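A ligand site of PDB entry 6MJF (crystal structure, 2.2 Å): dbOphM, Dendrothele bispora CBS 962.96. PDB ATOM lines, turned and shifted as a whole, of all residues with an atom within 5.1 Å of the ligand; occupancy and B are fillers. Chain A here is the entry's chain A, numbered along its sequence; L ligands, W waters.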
ATOM      1  N   ILE A  19      27.730 -30.342 -16.236  1.00  0.00           N
ATOM      2  CA  ILE A  19      27.972 -31.111 -17.457  1.00  0.00           C
ATOM      3  C   ILE A  19      28.612 -32.449 -17.109  1.00  0.00           C
ATOM      4  O   ILE A  19      28.068 -33.509 -17.462  1.00  0.00           O
ATOM      5  CB  ILE A  19      28.830 -30.321 -18.445  1.00  0.00           C
ATOM      6  CG1 ILE A  19      28.128 -29.016 -18.833  1.00  0.00           C
ATOM      7  CG2 ILE A  19      29.117 -31.157 -19.682  1.00  0.00           C
ATOM      8  CD1 ILE A  19      26.795 -29.225 -19.531  1.00  0.00           C
ATOM      9  N   ILE A  44      21.430 -36.276 -19.744  1.00  0.00           N
ATOM     10  CA  ILE A  44      21.859 -37.134 -20.846  1.00  0.00           C
ATOM     11  C   ILE A  44      23.085 -37.937 -20.442  1.00  0.00           C
ATOM     12  O   ILE A  44      23.898 -38.321 -21.284  1.00  0.00           O
ATOM     13  CB  ILE A  44      22.138 -36.290 -22.109  1.00  0.00           C
ATOM     14  CG1 ILE A  44      23.228 -35.254 -21.834  1.00  0.00           C
ATOM     15  CG2 ILE A  44      20.861 -35.616 -22.596  1.00  0.00           C
ATOM     16  CD1 ILE A  44      23.570 -34.417 -23.036  1.00  0.00           C
ATOM     17  N   TYR A  98      20.258 -30.789 -17.216  1.00  0.00           N
ATOM     18  CA  TYR A  98      21.697 -30.882 -17.065  1.00  0.00           C
ATOM     19  C   TYR A  98      22.375 -29.561 -17.423  1.00  0.00           C
ATOM     20  O   TYR A  98      21.833 -28.728 -18.168  1.00  0.00           O
ATOM     21  CB  TYR A  98      22.253 -32.025 -17.928  1.00  0.00           C
ATOM     22  CG  TYR A  98      22.350 -31.727 -19.398  1.00  0.00           C
ATOM     23  CD1 TYR A  98      21.272 -31.968 -20.252  1.00  0.00           C
ATOM     24  CD2 TYR A  98      23.514 -31.222 -19.963  1.00  0.00           C
ATOM     25  CE1 TYR A  98      21.348 -31.705 -21.606  1.00  0.00           C
ATOM     26  CE2 TYR A  98      23.608 -30.960 -21.311  1.00  0.00           C
ATOM     27  CZ  TYR A  98      22.519 -31.205 -22.131  1.00  0.00           C
ATOM     28  OH  TYR A  98      22.613 -30.943 -23.479  1.00  0.00           O
ATOM     29  N   GLY A  99      23.570 -29.367 -16.877  1.00  0.00           N
ATOM     30  CA  GLY A  99      24.250 -28.093 -17.065  1.00  0.00           C
ATOM     31  C   GLY A  99      23.582 -27.003 -16.252  1.00  0.00           C
ATOM     32  O   GLY A  99      23.141 -27.214 -15.120  1.00  0.00           O
ATOM     33  N   HIS A 100      23.520 -25.807 -16.844  1.00  0.00           N
ATOM     34  CA  HIS A 100      22.758 -24.712 -16.275  1.00  0.00           C
ATOM     35  C   HIS A 100      21.326 -24.810 -16.768  1.00  0.00           C
ATOM     36  O   HIS A 100      21.100 -24.797 -17.990  1.00  0.00           O
ATOM     37  CB  HIS A 100      23.376 -23.375 -16.670  1.00  0.00           C
ATOM     38  CG  HIS A 100      22.747 -22.183 -16.017  1.00  0.00           C
ATOM     39  ND1 HIS A 100      21.443 -21.805 -16.249  1.00  0.00           N
ATOM     40  CD2 HIS A 100      23.263 -21.276 -15.151  1.00  0.00           C
ATOM     41  CE1 HIS A 100      21.172 -20.718 -15.537  1.00  0.00           C
ATOM     42  NE2 HIS A 100      22.255 -20.375 -14.870  1.00  0.00           N
ATOM     43  N   VAL A 103      20.140 -22.188 -19.484  1.00  0.00           N
ATOM     44  CA  VAL A 103      21.050 -21.875 -20.581  1.00  0.00           C
ATOM     45  C   VAL A 103      20.725 -22.824 -21.722  1.00  0.00           C
ATOM     46  O   VAL A 103      20.987 -24.028 -21.639  1.00  0.00           O
ATOM     47  CB  VAL A 103      22.521 -21.995 -20.131  1.00  0.00           C
ATOM     48  CG1 VAL A 103      23.444 -22.002 -21.333  1.00  0.00           C
ATOM     49  CG2 VAL A 103      22.874 -20.854 -19.198  1.00  0.00           C
ATOM     50  N   PHE A 104      20.150 -22.271 -22.795  1.00  0.00           N
ATOM     51  CA  PHE A 104      19.714 -23.045 -23.960  1.00  0.00           C
ATOM     52  C   PHE A 104      18.750 -24.161 -23.553  1.00  0.00           C
ATOM     53  O   PHE A 104      18.874 -25.315 -23.973  1.00  0.00           O
ATOM     54  CB  PHE A 104      20.910 -23.597 -24.736  1.00  0.00           C
ATOM     55  CG  PHE A 104      21.750 -22.537 -25.399  1.00  0.00           C
ATOM     56  CD1 PHE A 104      22.690 -21.828 -24.676  1.00  0.00           C
ATOM     57  CD2 PHE A 104      21.579 -22.238 -26.745  1.00  0.00           C
ATOM     58  CE1 PHE A 104      23.454 -20.846 -25.284  1.00  0.00           C
ATOM     59  CE2 PHE A 104      22.332 -21.248 -27.351  1.00  0.00           C
ATOM     60  CZ  PHE A 104      23.278 -20.560 -26.616  1.00  0.00           C
ATOM     61  N   VAL A 105      17.778 -23.803 -22.713  1.00  0.00           N
ATOM     62  CA  VAL A 105      16.754 -24.720 -22.231  1.00  0.00           C
ATOM     63  C   VAL A 105      15.418 -24.006 -22.335  1.00  0.00           C
ATOM     64  O   VAL A 105      15.178 -23.020 -21.635  1.00  0.00           O
ATOM     65  CB  VAL A 105      17.009 -25.175 -20.782  1.00  0.00           C
ATOM     66  CG1 VAL A 105      15.896 -26.109 -20.323  1.00  0.00           C
ATOM     67  CG2 VAL A 105      18.363 -25.854 -20.667  1.00  0.00           C
ATOM     68  N   VAL A 128      26.410 -25.194 -13.597  1.00  0.00           N
ATOM     69  CA  VAL A 128      27.579 -25.111 -14.464  1.00  0.00           C
ATOM     70  C   VAL A 128      27.166 -25.455 -15.889  1.00  0.00           C
ATOM     71  O   VAL A 128      26.721 -26.565 -16.165  1.00  0.00           O
ATOM     72  CB  VAL A 128      28.693 -26.044 -13.969  1.00  0.00           C
ATOM     73  CG1 VAL A 128      29.777 -26.174 -15.037  1.00  0.00           C
ATOM     74  CG2 VAL A 128      29.271 -25.548 -12.665  1.00  0.00           C
ATOM     75  N   SER A 129      27.324 -24.496 -16.797  1.00  0.00           N
ATOM     76  CA  SER A 129      26.914 -24.688 -18.180  1.00  0.00           C
ATOM     77  C   SER A 129      28.058 -25.255 -19.019  1.00  0.00           C
ATOM     78  O   SER A 129      29.196 -25.397 -18.564  1.00  0.00           O
ATOM     79  CB  SER A 129      26.413 -23.373 -18.777  1.00  0.00           C
ATOM     80  OG  SER A 129      27.488 -22.514 -19.109  1.00  0.00           O
ATOM     81  N   ALA A 130      27.745 -25.580 -20.274  1.00  0.00           N
ATOM     82  CA  ALA A 130      28.777 -26.010 -21.201  1.00  0.00           C
ATOM     83  C   ALA A 130      29.730 -24.868 -21.545  1.00  0.00           C
ATOM     84  O   ALA A 130      30.899 -25.106 -21.846  1.00  0.00           O
ATOM     85  CB  ALA A 130      28.157 -26.574 -22.484  1.00  0.00           C
ATOM     86  N   GLU A 131      29.225 -23.628 -21.507  1.00  0.00           N
ATOM     87  CA  GLU A 131      30.100 -22.479 -21.691  1.00  0.00           C
ATOM     88  C   GLU A 131      31.072 -22.341 -20.521  1.00  0.00           C
ATOM     89  O   GLU A 131      32.249 -22.014 -20.721  1.00  0.00           O
ATOM     90  CB  GLU A 131      29.259 -21.209 -21.840  1.00  0.00           C
ATOM     91  CG  GLU A 131      30.076 -19.941 -21.995  1.00  0.00           C
ATOM     92  CD  GLU A 131      29.265 -18.798 -22.574  1.00  0.00           C
ATOM     93  OE1 GLU A 131      28.729 -18.952 -23.688  1.00  0.00           O
ATOM     94  OE2 GLU A 131      29.159 -17.744 -21.915  1.00  0.00           O
ATOM     95  N   LEU A 170      29.258 -20.743 -30.136  1.00  0.00           N
ATOM     96  CA  LEU A 170      28.075 -21.182 -30.860  1.00  0.00           C
ATOM     97  C   LEU A 170      27.588 -22.494 -30.263  1.00  0.00           C
ATOM     98  O   LEU A 170      28.316 -23.490 -30.274  1.00  0.00           O
ATOM     99  CB  LEU A 170      28.351 -21.338 -32.351  1.00  0.00           C
ATOM    100  CG  LEU A 170      28.731 -20.073 -33.132  1.00  0.00           C
ATOM    101  CD1 LEU A 170      29.171 -20.439 -34.541  1.00  0.00           C
ATOM    102  CD2 LEU A 170      27.570 -19.088 -33.159  1.00  0.00           C
ATOM    103  N   PHE A 171      26.363 -22.495 -29.738  1.00  0.00           N
ATOM    104  CA  PHE A 171      25.712 -23.704 -29.267  1.00  0.00           C
ATOM    105  C   PHE A 171      24.940 -24.363 -30.401  1.00  0.00           C
ATOM    106  O   PHE A 171      24.548 -23.723 -31.379  1.00  0.00           O
ATOM    107  CB  PHE A 171      24.756 -23.400 -28.116  1.00  0.00           C
ATOM    108  CG  PHE A 171      25.408 -23.303 -26.769  1.00  0.00           C
ATOM    109  CD1 PHE A 171      26.338 -22.308 -26.494  1.00  0.00           C
ATOM    110  CD2 PHE A 171      25.059 -24.180 -25.761  1.00  0.00           C
ATOM    111  CE1 PHE A 171      26.922 -22.220 -25.252  1.00  0.00           C
ATOM    112  CE2 PHE A 171      25.638 -24.091 -24.506  1.00  0.00           C
ATOM    113  CZ  PHE A 171      26.575 -23.104 -24.250  1.00  0.00           C
ATOM    114  N   GLN A 172      24.714 -25.674 -30.239  1.00  0.00           N
ATOM    115  CA  GLN A 172      23.818 -26.424 -31.123  1.00  0.00           C
ATOM    116  C   GLN A 172      24.273 -26.361 -32.584  1.00  0.00           C
ATOM    117  O   GLN A 172      23.453 -26.302 -33.500  1.00  0.00           O
ATOM    118  CB  GLN A 172      22.370 -25.965 -30.969  1.00  0.00           C
ATOM    119  CG  GLN A 172      21.916 -25.858 -29.521  1.00  0.00           C
ATOM    120  CD  GLN A 172      20.416 -25.864 -29.362  1.00  0.00           C
ATOM    121  OE1 GLN A 172      19.875 -26.568 -28.510  1.00  0.00           O
ATOM    122  NE2 GLN A 172      19.720 -25.082 -30.187  1.00  0.00           N
ATOM    123  N   VAL A 173      25.590 -26.383 -32.798  1.00  0.00           N
ATOM    124  CA  VAL A 173      26.119 -26.468 -34.154  1.00  0.00           C
ATOM    125  C   VAL A 173      25.900 -27.846 -34.773  1.00  0.00           C
ATOM    126  O   VAL A 173      26.166 -28.026 -35.965  1.00  0.00           O
ATOM    127  CB  VAL A 173      27.624 -26.142 -34.172  1.00  0.00           C
ATOM    128  CG1 VAL A 173      27.858 -24.697 -33.740  1.00  0.00           C
ATOM    129  CG2 VAL A 173      28.398 -27.109 -33.289  1.00  0.00           C
ATOM    130  N   TYR A 211      34.570 -28.165 -29.548  1.00  0.00           N
ATOM    131  CA  TYR A 211      34.635 -28.410 -28.108  1.00  0.00           C
ATOM    132  C   TYR A 211      33.530 -29.360 -27.674  1.00  0.00           C
ATOM    133  O   TYR A 211      32.358 -29.151 -27.996  1.00  0.00           O
ATOM    134  CB  TYR A 211      34.534 -27.108 -27.316  1.00  0.00           C
ATOM    135  CG  TYR A 211      34.542 -27.325 -25.831  1.00  0.00           C
ATOM    136  CD1 TYR A 211      35.661 -27.830 -25.180  1.00  0.00           C
ATOM    137  CD2 TYR A 211      33.421 -27.041 -25.059  1.00  0.00           C
ATOM    138  CE1 TYR A 211      35.672 -28.034 -23.823  1.00  0.00           C
ATOM    139  CE2 TYR A 211      33.420 -27.251 -23.698  1.00  0.00           C
ATOM    140  CZ  TYR A 211      34.554 -27.745 -23.088  1.00  0.00           C
ATOM    141  OH  TYR A 211      34.571 -27.956 -21.720  1.00  0.00           O
ATOM    142  N   ILE A 212      33.911 -30.404 -26.945  1.00  0.00           N
ATOM    143  CA  ILE A 212      32.981 -31.316 -26.281  1.00  0.00           C
ATOM    144  C   ILE A 212      33.551 -31.602 -24.893  1.00  0.00           C
ATOM    145  O   ILE A 212      34.542 -32.322 -24.774  1.00  0.00           O
ATOM    146  CB  ILE A 212      32.755 -32.625 -27.051  1.00  0.00           C
ATOM    147  CG1 ILE A 212      32.318 -32.357 -28.487  1.00  0.00           C
ATOM    148  CG2 ILE A 212      31.725 -33.485 -26.335  1.00  0.00           C
ATOM    149  CD1 ILE A 212      32.147 -33.617 -29.317  1.00  0.00           C
ATOM    150  N   ALA A 213      32.937 -31.028 -23.870  1.00  0.00           N
ATOM    151  CA  ALA A 213      33.367 -31.293 -22.503  1.00  0.00           C
ATOM    152  C   ALA A 213      33.178 -32.765 -22.165  1.00  0.00           C
ATOM    153  O   ALA A 213      32.233 -33.424 -22.631  1.00  0.00           O
ATOM    154  CB  ALA A 213      32.574 -30.433 -21.513  1.00  0.00           C
ATOM    155  N   MET A 215      31.897 -35.822 -20.331  1.00  0.00           N
ATOM    156  CA  MET A 215      30.696 -36.085 -19.543  1.00  0.00           C
ATOM    157  C   MET A 215      30.941 -37.098 -18.429  1.00  0.00           C
ATOM    158  O   MET A 215      30.174 -37.122 -17.463  1.00  0.00           O
ATOM    159  CB  MET A 215      29.575 -36.581 -20.451  1.00  0.00           C
ATOM    160  CG  MET A 215      28.607 -35.498 -20.893  1.00  0.00           C
ATOM    161  SD  MET A 215      27.377 -36.075 -22.073  1.00  0.00           S
ATOM    162  CE  MET A 215      28.286 -35.966 -23.612  1.00  0.00           C
ATOM    163  N   GLY A 242      25.283 -33.696 -31.136  1.00  0.00           N
ATOM    164  CA  GLY A 242      24.321 -32.998 -30.289  1.00  0.00           C
ATOM    165  C   GLY A 242      24.915 -32.323 -29.069  1.00  0.00           C
ATOM    166  O   GLY A 242      24.264 -31.454 -28.480  1.00  0.00           O
ATOM    167  N   VAL A 243      26.126 -32.707 -28.666  1.00  0.00           N
ATOM    168  CA  VAL A 243      26.759 -32.094 -27.502  1.00  0.00           C
ATOM    169  C   VAL A 243      28.022 -31.359 -27.931  1.00  0.00           C
ATOM    170  O   VAL A 243      28.961 -31.214 -27.148  1.00  0.00           O
ATOM    171  CB  VAL A 243      27.061 -33.133 -26.403  1.00  0.00           C
ATOM    172  CG1 VAL A 243      25.762 -33.672 -25.823  1.00  0.00           C
ATOM    173  CG2 VAL A 243      27.914 -34.255 -26.961  1.00  0.00           C
ATOM    174  N   SER A 244      28.046 -30.896 -29.177  1.00  0.00           N
ATOM    175  CA  SER A 244      29.185 -30.189 -29.737  1.00  0.00           C
ATOM    176  C   SER A 244      28.982 -28.674 -29.652  1.00  0.00           C
ATOM    177  O   SER A 244      27.881 -28.175 -29.905  1.00  0.00           O
ATOM    178  CB  SER A 244      29.424 -30.602 -31.183  1.00  0.00           C
ATOM    179  OG  SER A 244      30.016 -31.892 -31.262  1.00  0.00           O
ATOM    180  N   THR A 245      30.048 -27.960 -29.314  1.00  0.00           N
ATOM    181  CA  THR A 245      30.038 -26.507 -29.240  1.00  0.00           C
ATOM    182  C   THR A 245      31.277 -25.979 -29.953  1.00  0.00           C
ATOM    183  O   THR A 245      32.361 -26.550 -29.843  1.00  0.00           O
ATOM    184  CB  THR A 245      29.999 -26.014 -27.783  1.00  0.00           C
ATOM    185  OG1 THR A 245      28.772 -26.421 -27.180  1.00  0.00           O
ATOM    186  CG2 THR A 245      30.117 -24.505 -27.705  1.00  0.00           C
HETATM  187  N1  LIG L   1      21.747 -26.472 -20.552  1.00  0.00           N
HETATM  188  C1  LIG L   1      22.959 -26.933 -21.210  1.00  0.00           C
HETATM  189  C2  LIG L   1      22.826 -26.837 -22.714  1.00  0.00           C
HETATM  190  C3  LIG L   1      21.723 -27.693 -23.324  1.00  0.00           C
HETATM  191  S1  LIG L   1      21.273 -27.168 -24.997  1.00  0.00           S
HETATM  192  C4  LIG L   1      24.171 -26.148 -20.736  1.00  0.00           C
HETATM  193  O1  LIG L   1      25.149 -25.982 -21.474  1.00  0.00           O
HETATM  194  O2  LIG L   1      24.205 -25.658 -19.606  1.00  0.00           O
HETATM  195  C5  LIG L   1      22.431 -28.354 -25.735  1.00  0.00           C
HETATM  196  C6  LIG L   1      23.673 -27.668 -26.288  1.00  0.00           C
HETATM  197  O3  LIG L   1      24.591 -27.407 -25.251  1.00  0.00           O
HETATM  198  C7  LIG L   1      24.415 -28.512 -27.312  1.00  0.00           C
HETATM  199  O4  LIG L   1      23.965 -28.272 -28.624  1.00  0.00           O
HETATM  200  C8  LIG L   1      25.848 -28.093 -27.145  1.00  0.00           C
HETATM  201  O5  LIG L   1      26.127 -26.973 -27.957  1.00  0.00           O
HETATM  202  C9  LIG L   1      25.914 -27.663 -25.691  1.00  0.00           C
HETATM  203  N2  LIG L   1      26.490 -28.781 -24.926  1.00  0.00           N
HETATM  204  C10 LIG L   1      25.798 -29.749 -24.248  1.00  0.00           C
HETATM  205  N3  LIG L   1      26.686 -30.608 -23.703  1.00  0.00           N
HETATM  206  C11 LIG L   1      27.932 -30.200 -24.029  1.00  0.00           C
HETATM  207  C12 LIG L   1      29.188 -30.706 -23.736  1.00  0.00           C
HETATM  208  N4  LIG L   1      29.317 -31.798 -22.994  1.00  0.00           N
HETATM  209  N5  LIG L   1      30.308 -30.065 -24.222  1.00  0.00           N
HETATM  210  C13 LIG L   1      30.180 -28.925 -24.990  1.00  0.00           C
HETATM  211  N6  LIG L   1      28.923 -28.433 -25.282  1.00  0.00           N
HETATM  212  C14 LIG L   1      27.826 -29.061 -24.804  1.00  0.00           C
HETATM  213  O   HOH W   1      26.855 -32.861 -22.034  1.00  0.00           O
HETATM  214  O   HOH W   2      25.671 -29.379 -31.055  1.00  0.00           O
HETATM  215  O   HOH W   3      20.056 -28.766 -20.410  1.00  0.00           O
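Water W1 lies within hydrogen-bond range of a nitrogen (N3) of the ligand (2.8 Å) and the side-chain sulfur (SD) of Met 215 (3.3 Å).
Water W3 lies within hydrogen-bond range of N1 of the ligand (2.9 Å) and O of Tyr 98 (2.9 Å).
Water W2 lies within hydrogen-bond range of the backbone carbonyl oxygen of Ser 244 (2.8 Å), an oxygen (O4) of the ligand (3.2 Å) and the backbone NH of Val 173 (3.5 Å).
The backbone carbonyl oxygen (O) of Thr 245 lies within hydrogen-bond range of the backbone NH (N) of Tyr 211, at 2.8 Å.
The backbone NH (N) of His 100 sits at hydrogen-bond distance from the backbone carbonyl oxygen (O) of Val 128.
The side-chain hydroxyl (OG) of Ser 129 sits at hydrogen-bond distance from the backbone NH (N) of Glu 131 (3.2 Å).
S1 of the ligand lies close to O of Phe 104 (3.2 Å).
The backbone carbonyl oxygen (O) of Val 243 sits close to a nitrogen (N6) of the ligand.
Residues that only touch the ligand: Ser 129, Phe 171, Ile 19, Val 105, Gly 99, Ile 212 and Tyr 211.
Hydrophobic or aromatic side chains within 4 Å of the ligand: Ile 19, Tyr 98, His 100, Phe 104, Val 105, Ala 130, Phe 171, Tyr 211, Ala 213 and Val 243.
Of the 24 residues printed, 18 come within 4 Å of the ligand.
A nitrogen (N6) of the ligand lies within hydrogen-bond range of the side-chain hydroxyl of Thr 245.
The backbone carbonyl oxygen (O) of Val 103 lies within hydrogen-bond range of a nitrogen (N1) of the ligand, at 2.8 Å.
N5 of the ligand is in hydrogen-bond range of N of Ala 213, 2.8 Å away.
A nitrogen (N4) of the ligand lies within hydrogen-bond range of the backbone carbonyl oxygen (O) of Ala 213 (3.4 Å).
The backbone NH of His 100 is in hydrogen-bond range of an oxygen (O2) of the ligand (2.8 Å).
A nitrogen (N1) of the ligand sits at hydrogen-bond distance from the backbone carbonyl oxygen of His 100 (3.1 Å).
O of Ser 244 lies within hydrogen-bond range of O5 of the ligand (2.9 Å).
N of Ala 130 is in hydrogen-bond range of O1 of the ligand.
The backbone NH (N) of Gln 172 lies within hydrogen-bond range of an oxygen (O5) of the ligand (3.0 Å).
O of Gly 242 lies close to O4 of the ligand (3.2 Å).
A nitrogen (N1) of the ligand is in hydrogen-bond range of the backbone carbonyl oxygen (O) of Tyr 98, 3.3 Å away.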
